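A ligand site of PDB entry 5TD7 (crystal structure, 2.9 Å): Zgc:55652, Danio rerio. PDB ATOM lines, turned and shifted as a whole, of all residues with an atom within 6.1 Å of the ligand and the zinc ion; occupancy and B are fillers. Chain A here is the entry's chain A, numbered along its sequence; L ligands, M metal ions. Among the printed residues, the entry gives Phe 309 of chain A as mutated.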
ATOM      1  N   ALA A  26     -22.785  -3.867 -11.924  1.00  0.00           N
ATOM      2  CA  ALA A  26     -22.296  -2.874 -12.860  1.00  0.00           C
ATOM      3  C   ALA A  26     -21.047  -2.178 -12.363  1.00  0.00           C
ATOM      4  O   ALA A  26     -20.182  -1.803 -13.170  1.00  0.00           O
ATOM      5  CB  ALA A  26     -23.377  -1.835 -13.151  1.00  0.00           C
ATOM      6  N   ILE A  29     -16.341  -3.584 -10.895  1.00  0.00           N
ATOM      7  CA  ILE A  29     -15.013  -3.529 -11.489  1.00  0.00           C
ATOM      8  C   ILE A  29     -14.237  -2.290 -11.052  1.00  0.00           C
ATOM      9  O   ILE A  29     -13.018  -2.263 -11.213  1.00  0.00           O
ATOM     10  CB  ILE A  29     -15.089  -3.574 -13.020  1.00  0.00           C
ATOM     11  CG1 ILE A  29     -15.994  -2.455 -13.526  1.00  0.00           C
ATOM     12  CG2 ILE A  29     -15.587  -4.934 -13.477  1.00  0.00           C
ATOM     13  CD1 ILE A  29     -15.938  -2.266 -15.026  1.00  0.00           C
ATOM     14  N   GLU A  30     -14.903  -1.268 -10.515  1.00  0.00           N
ATOM     15  CA  GLU A  30     -14.225  -0.033 -10.111  1.00  0.00           C
ATOM     16  C   GLU A  30     -13.831  -0.167  -8.649  1.00  0.00           C
ATOM     17  O   GLU A  30     -14.618   0.104  -7.729  1.00  0.00           O
ATOM     18  CB  GLU A  30     -15.128   1.181 -10.337  1.00  0.00           C
ATOM     19  CG  GLU A  30     -14.372   2.429 -10.733  1.00  0.00           C
ATOM     20  CD  GLU A  30     -13.405   2.898  -9.669  1.00  0.00           C
ATOM     21  OE1 GLU A  30     -13.806   2.940  -8.485  1.00  0.00           O
ATOM     22  OE2 GLU A  30     -12.240   3.219 -10.007  1.00  0.00           O
ATOM     23  N   ARG A  34      -7.237  -0.446  -8.275  1.00  0.00           N
ATOM     24  CA  ARG A  34      -6.766   0.129  -9.530  1.00  0.00           C
ATOM     25  C   ARG A  34      -5.723   1.208  -9.280  1.00  0.00           C
ATOM     26  O   ARG A  34      -4.749   1.336 -10.036  1.00  0.00           O
ATOM     27  CB  ARG A  34      -7.933   0.707 -10.320  1.00  0.00           C
ATOM     28  CG  ARG A  34      -9.113  -0.248 -10.522  1.00  0.00           C
ATOM     29  CD  ARG A  34     -10.022   0.253 -11.650  1.00  0.00           C
ATOM     30  NE  ARG A  34     -10.370   1.660 -11.510  1.00  0.00           N
ATOM     31  CZ  ARG A  34      -9.921   2.635 -12.286  1.00  0.00           C
ATOM     32  NH1 ARG A  34      -9.105   2.359 -13.298  1.00  0.00           N
ATOM     33  NH2 ARG A  34     -10.299   3.894 -12.062  1.00  0.00           N
ATOM     34  N   ASP A  96     -25.025   3.950 -13.445  1.00  0.00           N
ATOM     35  CA  ASP A  96     -23.781   3.178 -13.237  1.00  0.00           C
ATOM     36  C   ASP A  96     -22.728   3.982 -12.477  1.00  0.00           C
ATOM     37  O   ASP A  96     -21.655   4.305 -12.983  1.00  0.00           O
ATOM     38  CB  ASP A  96     -23.223   2.697 -14.581  1.00  0.00           C
ATOM     39  CG  ASP A  96     -24.212   1.842 -15.347  1.00  0.00           C
ATOM     40  OD1 ASP A  96     -24.365   0.654 -15.004  1.00  0.00           O
ATOM     41  OD2 ASP A  96     -24.832   2.375 -16.298  1.00  0.00           O
ATOM     42  N   PRO A 136     -12.842   8.503 -11.825  1.00  0.00           N
ATOM     43  CA  PRO A 136     -12.580   9.004 -13.186  1.00  0.00           C
ATOM     44  C   PRO A 136     -13.429  10.226 -13.515  1.00  0.00           C
ATOM     45  O   PRO A 136     -14.135  10.762 -12.648  1.00  0.00           O
ATOM     46  CB  PRO A 136     -12.961   7.817 -14.071  1.00  0.00           C
ATOM     47  CG  PRO A 136     -13.160   6.649 -13.138  1.00  0.00           C
ATOM     48  CD  PRO A 136     -13.545   7.206 -11.835  1.00  0.00           C
ATOM     49  N   GLY A 137     -13.404  10.642 -14.781  1.00  0.00           N
ATOM     50  CA  GLY A 137     -14.021  11.902 -15.139  1.00  0.00           C
ATOM     51  C   GLY A 137     -14.922  11.927 -16.358  1.00  0.00           C
ATOM     52  O   GLY A 137     -15.991  12.537 -16.313  1.00  0.00           O
ATOM     53  N   HIS A 138     -14.509  11.297 -17.463  1.00  0.00           N
ATOM     54  CA  HIS A 138     -15.055  11.718 -18.761  1.00  0.00           C
ATOM     55  C   HIS A 138     -16.543  11.398 -18.951  1.00  0.00           C
ATOM     56  O   HIS A 138     -17.133  11.939 -19.892  1.00  0.00           O
ATOM     57  CB  HIS A 138     -14.221  11.136 -19.913  1.00  0.00           C
ATOM     58  CG  HIS A 138     -14.196   9.641 -19.966  1.00  0.00           C
ATOM     59  ND1 HIS A 138     -13.726   8.961 -21.066  1.00  0.00           N
ATOM     60  CD2 HIS A 138     -14.573   8.697 -19.075  1.00  0.00           C
ATOM     61  CE1 HIS A 138     -13.826   7.663 -20.850  1.00  0.00           C
ATOM     62  NE2 HIS A 138     -14.335   7.471 -19.647  1.00  0.00           N
ATOM     63  N   HIS A 139     -17.163  10.577 -18.103  1.00  0.00           N
ATOM     64  CA  HIS A 139     -18.613  10.376 -18.193  1.00  0.00           C
ATOM     65  C   HIS A 139     -19.404  11.373 -17.364  1.00  0.00           C
ATOM     66  O   HIS A 139     -20.616  11.495 -17.573  1.00  0.00           O
ATOM     67  CB  HIS A 139     -19.011   8.972 -17.729  1.00  0.00           C
ATOM     68  CG  HIS A 139     -18.337   7.864 -18.481  1.00  0.00           C
ATOM     69  ND1 HIS A 139     -18.267   7.843 -19.854  1.00  0.00           N
ATOM     70  CD2 HIS A 139     -17.727   6.738 -18.056  1.00  0.00           C
ATOM     71  CE1 HIS A 139     -17.640   6.750 -20.241  1.00  0.00           C
ATOM     72  NE2 HIS A 139     -17.292   6.063 -19.172  1.00  0.00           N
ATOM     73  N   ASN A 146     -22.139   9.904 -13.655  1.00  0.00           N
ATOM     74  CA  ASN A 146     -22.375   8.885 -14.662  1.00  0.00           C
ATOM     75  C   ASN A 146     -21.129   8.034 -14.828  1.00  0.00           C
ATOM     76  O   ASN A 146     -20.012   8.565 -14.863  1.00  0.00           O
ATOM     77  CB  ASN A 146     -22.761   9.529 -16.010  1.00  0.00           C
ATOM     78  CG  ASN A 146     -23.159   8.509 -17.058  1.00  0.00           C
ATOM     79  OD1 ASN A 146     -22.327   8.080 -17.874  1.00  0.00           O
ATOM     80  ND2 ASN A 146     -24.424   8.115 -17.064  1.00  0.00           N
ATOM     81  N   GLY A 147     -21.321   6.725 -14.952  1.00  0.00           N
ATOM     82  CA  GLY A 147     -20.233   5.816 -15.287  1.00  0.00           C
ATOM     83  C   GLY A 147     -19.017   5.964 -14.402  1.00  0.00           C
ATOM     84  O   GLY A 147     -17.935   6.312 -14.880  1.00  0.00           O
ATOM     85  N   PHE A 148     -19.195   5.746 -13.095  1.00  0.00           N
ATOM     86  CA  PHE A 148     -18.164   5.804 -12.061  1.00  0.00           C
ATOM     87  C   PHE A 148     -17.608   7.209 -11.850  1.00  0.00           C
ATOM     88  O   PHE A 148     -16.776   7.395 -10.942  1.00  0.00           O
ATOM     89  CB  PHE A 148     -16.994   4.851 -12.349  1.00  0.00           C
ATOM     90  CG  PHE A 148     -17.412   3.455 -12.718  1.00  0.00           C
ATOM     91  CD1 PHE A 148     -18.589   2.906 -12.235  1.00  0.00           C
ATOM     92  CD2 PHE A 148     -16.610   2.679 -13.545  1.00  0.00           C
ATOM     93  CE1 PHE A 148     -18.966   1.617 -12.568  1.00  0.00           C
ATOM     94  CE2 PHE A 148     -16.985   1.395 -13.887  1.00  0.00           C
ATOM     95  CZ  PHE A 148     -18.167   0.865 -13.393  1.00  0.00           C
ATOM     96  N   CYS A 149     -18.032   8.198 -12.626  1.00  0.00           N
ATOM     97  CA  CYS A 149     -17.478   9.546 -12.554  1.00  0.00           C
ATOM     98  C   CYS A 149     -18.380  10.465 -11.744  1.00  0.00           C
ATOM     99  O   CYS A 149     -19.611  10.361 -11.795  1.00  0.00           O
ATOM    100  CB  CYS A 149     -17.273  10.123 -13.950  1.00  0.00           C
ATOM    101  SG  CYS A 149     -16.347   9.066 -15.084  1.00  0.00           S
ATOM    102  N   ASP A 176      -9.515   6.064 -23.620  1.00  0.00           N
ATOM    103  CA  ASP A 176     -10.311   5.119 -22.854  1.00  0.00           C
ATOM    104  C   ASP A 176     -11.253   4.367 -23.797  1.00  0.00           C
ATOM    105  O   ASP A 176     -11.694   4.896 -24.823  1.00  0.00           O
ATOM    106  CB  ASP A 176     -11.084   5.880 -21.761  1.00  0.00           C
ATOM    107  CG  ASP A 176     -11.853   4.976 -20.835  1.00  0.00           C
ATOM    108  OD1 ASP A 176     -11.290   4.533 -19.819  1.00  0.00           O
ATOM    109  OD2 ASP A 176     -13.047   4.733 -21.115  1.00  0.00           O
ATOM    110  N   VAL A 177     -11.558   3.108 -23.478  1.00  0.00           N
ATOM    111  CA  VAL A 177     -12.375   2.310 -24.378  1.00  0.00           C
ATOM    112  C   VAL A 177     -13.835   2.753 -24.409  1.00  0.00           C
ATOM    113  O   VAL A 177     -14.569   2.358 -25.316  1.00  0.00           O
ATOM    114  CB  VAL A 177     -12.266   0.806 -24.033  1.00  0.00           C
ATOM    115  CG1 VAL A 177     -13.251   0.441 -22.937  1.00  0.00           C
ATOM    116  CG2 VAL A 177     -12.484  -0.051 -25.282  1.00  0.00           C
ATOM    117  N   HIS A 178     -14.267   3.552 -23.443  1.00  0.00           N
ATOM    118  CA  HIS A 178     -15.608   4.116 -23.403  1.00  0.00           C
ATOM    119  C   HIS A 178     -15.601   5.540 -23.950  1.00  0.00           C
ATOM    120  O   HIS A 178     -14.591   6.242 -23.881  1.00  0.00           O
ATOM    121  CB  HIS A 178     -16.182   4.148 -21.998  1.00  0.00           C
ATOM    122  CG  HIS A 178     -16.215   2.825 -21.314  1.00  0.00           C
ATOM    123  ND1 HIS A 178     -15.106   2.266 -20.723  1.00  0.00           N
ATOM    124  CD2 HIS A 178     -17.241   1.963 -21.104  1.00  0.00           C
ATOM    125  CE1 HIS A 178     -15.445   1.109 -20.185  1.00  0.00           C
ATOM    126  NE2 HIS A 178     -16.720   0.895 -20.404  1.00  0.00           N
ATOM    127  N   HIS A 179     -16.754   5.966 -24.451  1.00  0.00           N
ATOM    128  CA  HIS A 179     -16.884   7.328 -24.942  1.00  0.00           C
ATOM    129  C   HIS A 179     -17.026   8.284 -23.760  1.00  0.00           C
ATOM    130  O   HIS A 179     -17.734   8.001 -22.800  1.00  0.00           O
ATOM    131  CB  HIS A 179     -18.077   7.448 -25.877  1.00  0.00           C
ATOM    132  CG  HIS A 179     -18.263   8.813 -26.459  1.00  0.00           C
ATOM    133  ND1 HIS A 179     -19.459   9.497 -26.394  1.00  0.00           N
ATOM    134  CD2 HIS A 179     -17.403   9.627 -27.115  1.00  0.00           C
ATOM    135  CE1 HIS A 179     -19.328  10.670 -26.983  1.00  0.00           C
ATOM    136  NE2 HIS A 179     -18.085  10.771 -27.436  1.00  0.00           N
ATOM    137  N   TRP A 207     -22.528   0.178 -23.898  1.00  0.00           N
ATOM    138  CA  TRP A 207     -22.587   1.331 -22.972  1.00  0.00           C
ATOM    139  C   TRP A 207     -21.602   2.458 -23.327  1.00  0.00           C
ATOM    140  O   TRP A 207     -20.429   2.196 -23.607  1.00  0.00           O
ATOM    141  CB  TRP A 207     -22.314   0.846 -21.540  1.00  0.00           C
ATOM    142  CG  TRP A 207     -22.665   1.854 -20.494  1.00  0.00           C
ATOM    143  CD1 TRP A 207     -23.841   1.923 -19.799  1.00  0.00           C
ATOM    144  CD2 TRP A 207     -21.851   2.931 -20.029  1.00  0.00           C
ATOM    145  NE1 TRP A 207     -23.806   2.993 -18.941  1.00  0.00           N
ATOM    146  CE2 TRP A 207     -22.602   3.622 -19.055  1.00  0.00           C
ATOM    147  CE3 TRP A 207     -20.569   3.388 -20.335  1.00  0.00           C
ATOM    148  CZ2 TRP A 207     -22.103   4.740 -18.389  1.00  0.00           C
ATOM    149  CZ3 TRP A 207     -20.079   4.489 -19.680  1.00  0.00           C
ATOM    150  CH2 TRP A 207     -20.845   5.158 -18.723  1.00  0.00           C
ATOM    151  N   GLY A 267      -7.449   6.061 -20.354  1.00  0.00           N
ATOM    152  CA  GLY A 267      -8.060   4.866 -19.806  1.00  0.00           C
ATOM    153  C   GLY A 267      -7.453   3.651 -20.480  1.00  0.00           C
ATOM    154  O   GLY A 267      -7.291   3.621 -21.702  1.00  0.00           O
ATOM    155  N   ASP A 269      -8.615   0.472 -20.132  1.00  0.00           N
ATOM    156  CA  ASP A 269      -9.560  -0.582 -20.466  1.00  0.00           C
ATOM    157  C   ASP A 269      -9.610  -0.856 -21.964  1.00  0.00           C
ATOM    158  O   ASP A 269     -10.309  -1.774 -22.397  1.00  0.00           O
ATOM    159  CB  ASP A 269     -10.955  -0.222 -19.958  1.00  0.00           C
ATOM    160  CG  ASP A 269     -11.349   1.218 -20.264  1.00  0.00           C
ATOM    161  OD1 ASP A 269     -10.569   1.934 -20.922  1.00  0.00           O
ATOM    162  OD2 ASP A 269     -12.449   1.619 -19.854  1.00  0.00           O
ATOM    163  N   GLU A 276     -13.827  -5.196 -19.863  1.00  0.00           N
ATOM    164  CA  GLU A 276     -14.832  -4.240 -20.330  1.00  0.00           C
ATOM    165  C   GLU A 276     -14.601  -3.805 -21.770  1.00  0.00           C
ATOM    166  O   GLU A 276     -15.566  -3.679 -22.530  1.00  0.00           O
ATOM    167  CB  GLU A 276     -14.838  -3.025 -19.405  1.00  0.00           C
ATOM    168  CG  GLU A 276     -15.940  -2.042 -19.710  1.00  0.00           C
ATOM    169  CD  GLU A 276     -17.234  -2.350 -18.977  1.00  0.00           C
ATOM    170  OE1 GLU A 276     -18.213  -1.591 -19.192  1.00  0.00           O
ATOM    171  OE2 GLU A 276     -17.290  -3.335 -18.204  1.00  0.00           O
ATOM    172  N   GLU A 306      -8.169   7.444 -16.267  1.00  0.00           N
ATOM    173  CA  GLU A 306      -9.600   7.248 -16.397  1.00  0.00           C
ATOM    174  C   GLU A 306      -9.896   5.811 -16.005  1.00  0.00           C
ATOM    175  O   GLU A 306      -9.914   5.489 -14.812  1.00  0.00           O
ATOM    176  CB  GLU A 306     -10.082   7.592 -17.810  1.00  0.00           C
ATOM    177  CG  GLU A 306      -9.905   9.053 -18.210  1.00  0.00           C
ATOM    178  CD  GLU A 306     -11.064   9.946 -17.756  1.00  0.00           C
ATOM    179  OE1 GLU A 306     -11.947   9.465 -17.003  1.00  0.00           O
ATOM    180  OE2 GLU A 306     -11.115  11.127 -18.152  1.00  0.00           O
ATOM    181  N   GLY A 307     -10.133   4.913 -16.964  1.00  0.00           N
ATOM    182  CA  GLY A 307     -10.461   3.532 -16.673  1.00  0.00           C
ATOM    183  C   GLY A 307      -9.287   2.580 -16.854  1.00  0.00           C
ATOM    184  O   GLY A 307      -8.142   2.988 -17.073  1.00  0.00           O
ATOM    185  N   GLY A 308      -9.596   1.287 -16.767  1.00  0.00           N
ATOM    186  CA  GLY A 308      -8.622   0.215 -16.761  1.00  0.00           C
ATOM    187  C   GLY A 308      -8.879  -0.710 -15.590  1.00  0.00           C
ATOM    188  O   GLY A 308      -8.629  -0.328 -14.450  1.00  0.00           O
ATOM    189  N   PHE A 309      -9.400  -1.906 -15.849  1.00  0.00           N
ATOM    190  CA  PHE A 309     -10.000  -2.691 -14.776  1.00  0.00           C
ATOM    191  C   PHE A 309      -9.372  -4.056 -14.547  1.00  0.00           C
ATOM    192  O   PHE A 309      -9.656  -4.676 -13.520  1.00  0.00           O
ATOM    193  CB  PHE A 309     -11.509  -2.860 -15.034  1.00  0.00           C
ATOM    194  CG  PHE A 309     -12.216  -1.541 -15.187  1.00  0.00           C
ATOM    195  CD1 PHE A 309     -12.580  -0.814 -14.073  1.00  0.00           C
ATOM    196  CD2 PHE A 309     -12.488  -1.032 -16.440  1.00  0.00           C
ATOM    197  CE1 PHE A 309     -13.211   0.407 -14.199  1.00  0.00           C
ATOM    198  CE2 PHE A 309     -13.116   0.199 -16.583  1.00  0.00           C
ATOM    199  CZ  PHE A 309     -13.474   0.915 -15.464  1.00  0.00           C
HETATM  200  C1  LIG L   1     -24.861  -2.097 -17.289  1.00  0.00           C
HETATM  201  C2  LIG L   1     -23.783  -1.177 -17.959  1.00  0.00           C
HETATM  202  C3  LIG L   1     -22.482  -0.963 -17.114  1.00  0.00           C
HETATM  203  C4  LIG L   1     -20.331   0.278 -17.012  1.00  0.00           C
HETATM  204  C5  LIG L   1     -19.320   1.193 -17.815  1.00  0.00           C
HETATM  205  C6  LIG L   1     -18.328   2.003 -16.934  1.00  0.00           C
HETATM  206  C7  LIG L   1     -17.327   2.896 -17.741  1.00  0.00           C
HETATM  207  C8  LIG L   1     -16.368   3.763 -16.868  1.00  0.00           C
HETATM  208  C9  LIG L   1     -14.977   4.136 -17.545  1.00  0.00           C
HETATM  209  C10 LIG L   1     -14.141   5.131 -16.536  1.00  0.00           C
HETATM  210  F1  LIG L   1     -12.996   5.570 -17.161  1.00  0.00           F
HETATM  211  F2  LIG L   1     -14.879   6.227 -16.261  1.00  0.00           F
HETATM  212  F3  LIG L   1     -13.796   4.520 -15.387  1.00  0.00           F
HETATM  213  N1  LIG L   1     -21.436  -0.226 -17.887  1.00  0.00           N
HETATM  214  N2  LIG L   1     -26.154  -2.074 -18.005  1.00  0.00           N
HETATM  215  O1  LIG L   1     -15.158   4.918 -18.715  1.00  0.00           O
HETATM  216  O2  LIG L   1     -14.204   2.960 -17.789  1.00  0.00           O
HETATM  217 ZN    ZN M   1     -13.414   3.440 -19.676  1.00  0.00          ZN
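OD2 of Asp 176 binds the zinc ion.
OD2 of Asp 269 is bound to the zinc ion.
O2 of the ligand binds the zinc ion (2.1 Å).
The zinc ion is bound by ND1 of His 178, at 2.3 Å.
The zinc ion is bound by OD1 of Asp 176 (2.4 Å).
The zinc ion is bound by an oxygen (O1) of the ligand, 2.5 Å away.
The zinc ion has six donor atoms within binding distance.
Of the 25 residues printed, 3 come within 4 Å of the zinc ion.
O1 of the ligand sits close to NE2 of His 139 (2.5 Å).
A ring nitrogen (NE2) of His 138 lies close to an oxygen (O1) of the ligand (2.8 Å).
The side-chain carboxylate (OE1) of Glu 276 is in salt-bridge range of a nitrogen (N1) of the ligand (3.7 Å).
The side-chain carboxylate (OD2) of Asp 176 sits close to a ring nitrogen (NE2) of His 138, 3.4 Å away.
A ring nitrogen (NE2) of His 178 lies close to the side-chain carboxylate of Glu 276, at 3.1 Å.
The backbone NH (N) of His 138 lies within hydrogen-bond range of the side-chain carboxylate (OE1) of Glu 306, at 3.2 Å.
The backbone carbonyl oxygen (O) of Pro 136 lies close to the side-chain sulfur (SG) of Cys 149.
O of Asp 96 sits close to N of Gly 147 (3.1 Å).
NH2 of Arg 34 lies within hydrogen-bond range of O of Glu 306, 3.2 Å away.
OE1 of Glu 306 lies within hydrogen-bond range of N of Gly 137.
N of Gly 137 lies within hydrogen-bond range of SG of Cys 149.
F2 of the ligand sits close to O of Gly 147 (3.4 Å).
The side-chain sulfur (SG) of Cys 149 lies close to a fluorine (F2) of the ligand, 3.4 Å away.
The backbone NH (N) of Gly 307 lies close to a fluorine (F1) of the ligand, 2.9 Å away.
Asp 96 touches the ligand (OD1 to C3, 3.3 Å).
Pro 136 touches the ligand.
Phe 148 touches the ligand (CE2 to C6, 3.4 Å).
CG of Trp 207 touches N1 of the ligand (3.6 Å).
C of Glu 306 touches F1 of the ligand, at 3.3 Å.
Phe 309 touches the ligand.
Hydrophobic or aromatic side chains that line the ligand: Pro 136, His 138, His 139, Phe 148, His 178, Trp 207 and Phe 309.
15 residues have an atom within 4 Å of the ligand: Asp 96, Pro 136, His 138, His 139, Gly 147, Phe 148, Cys 149, Asp 176, His 178, Trp 207, Asp 269, Glu 276, Glu 306, Gly 307 and Phe 309.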
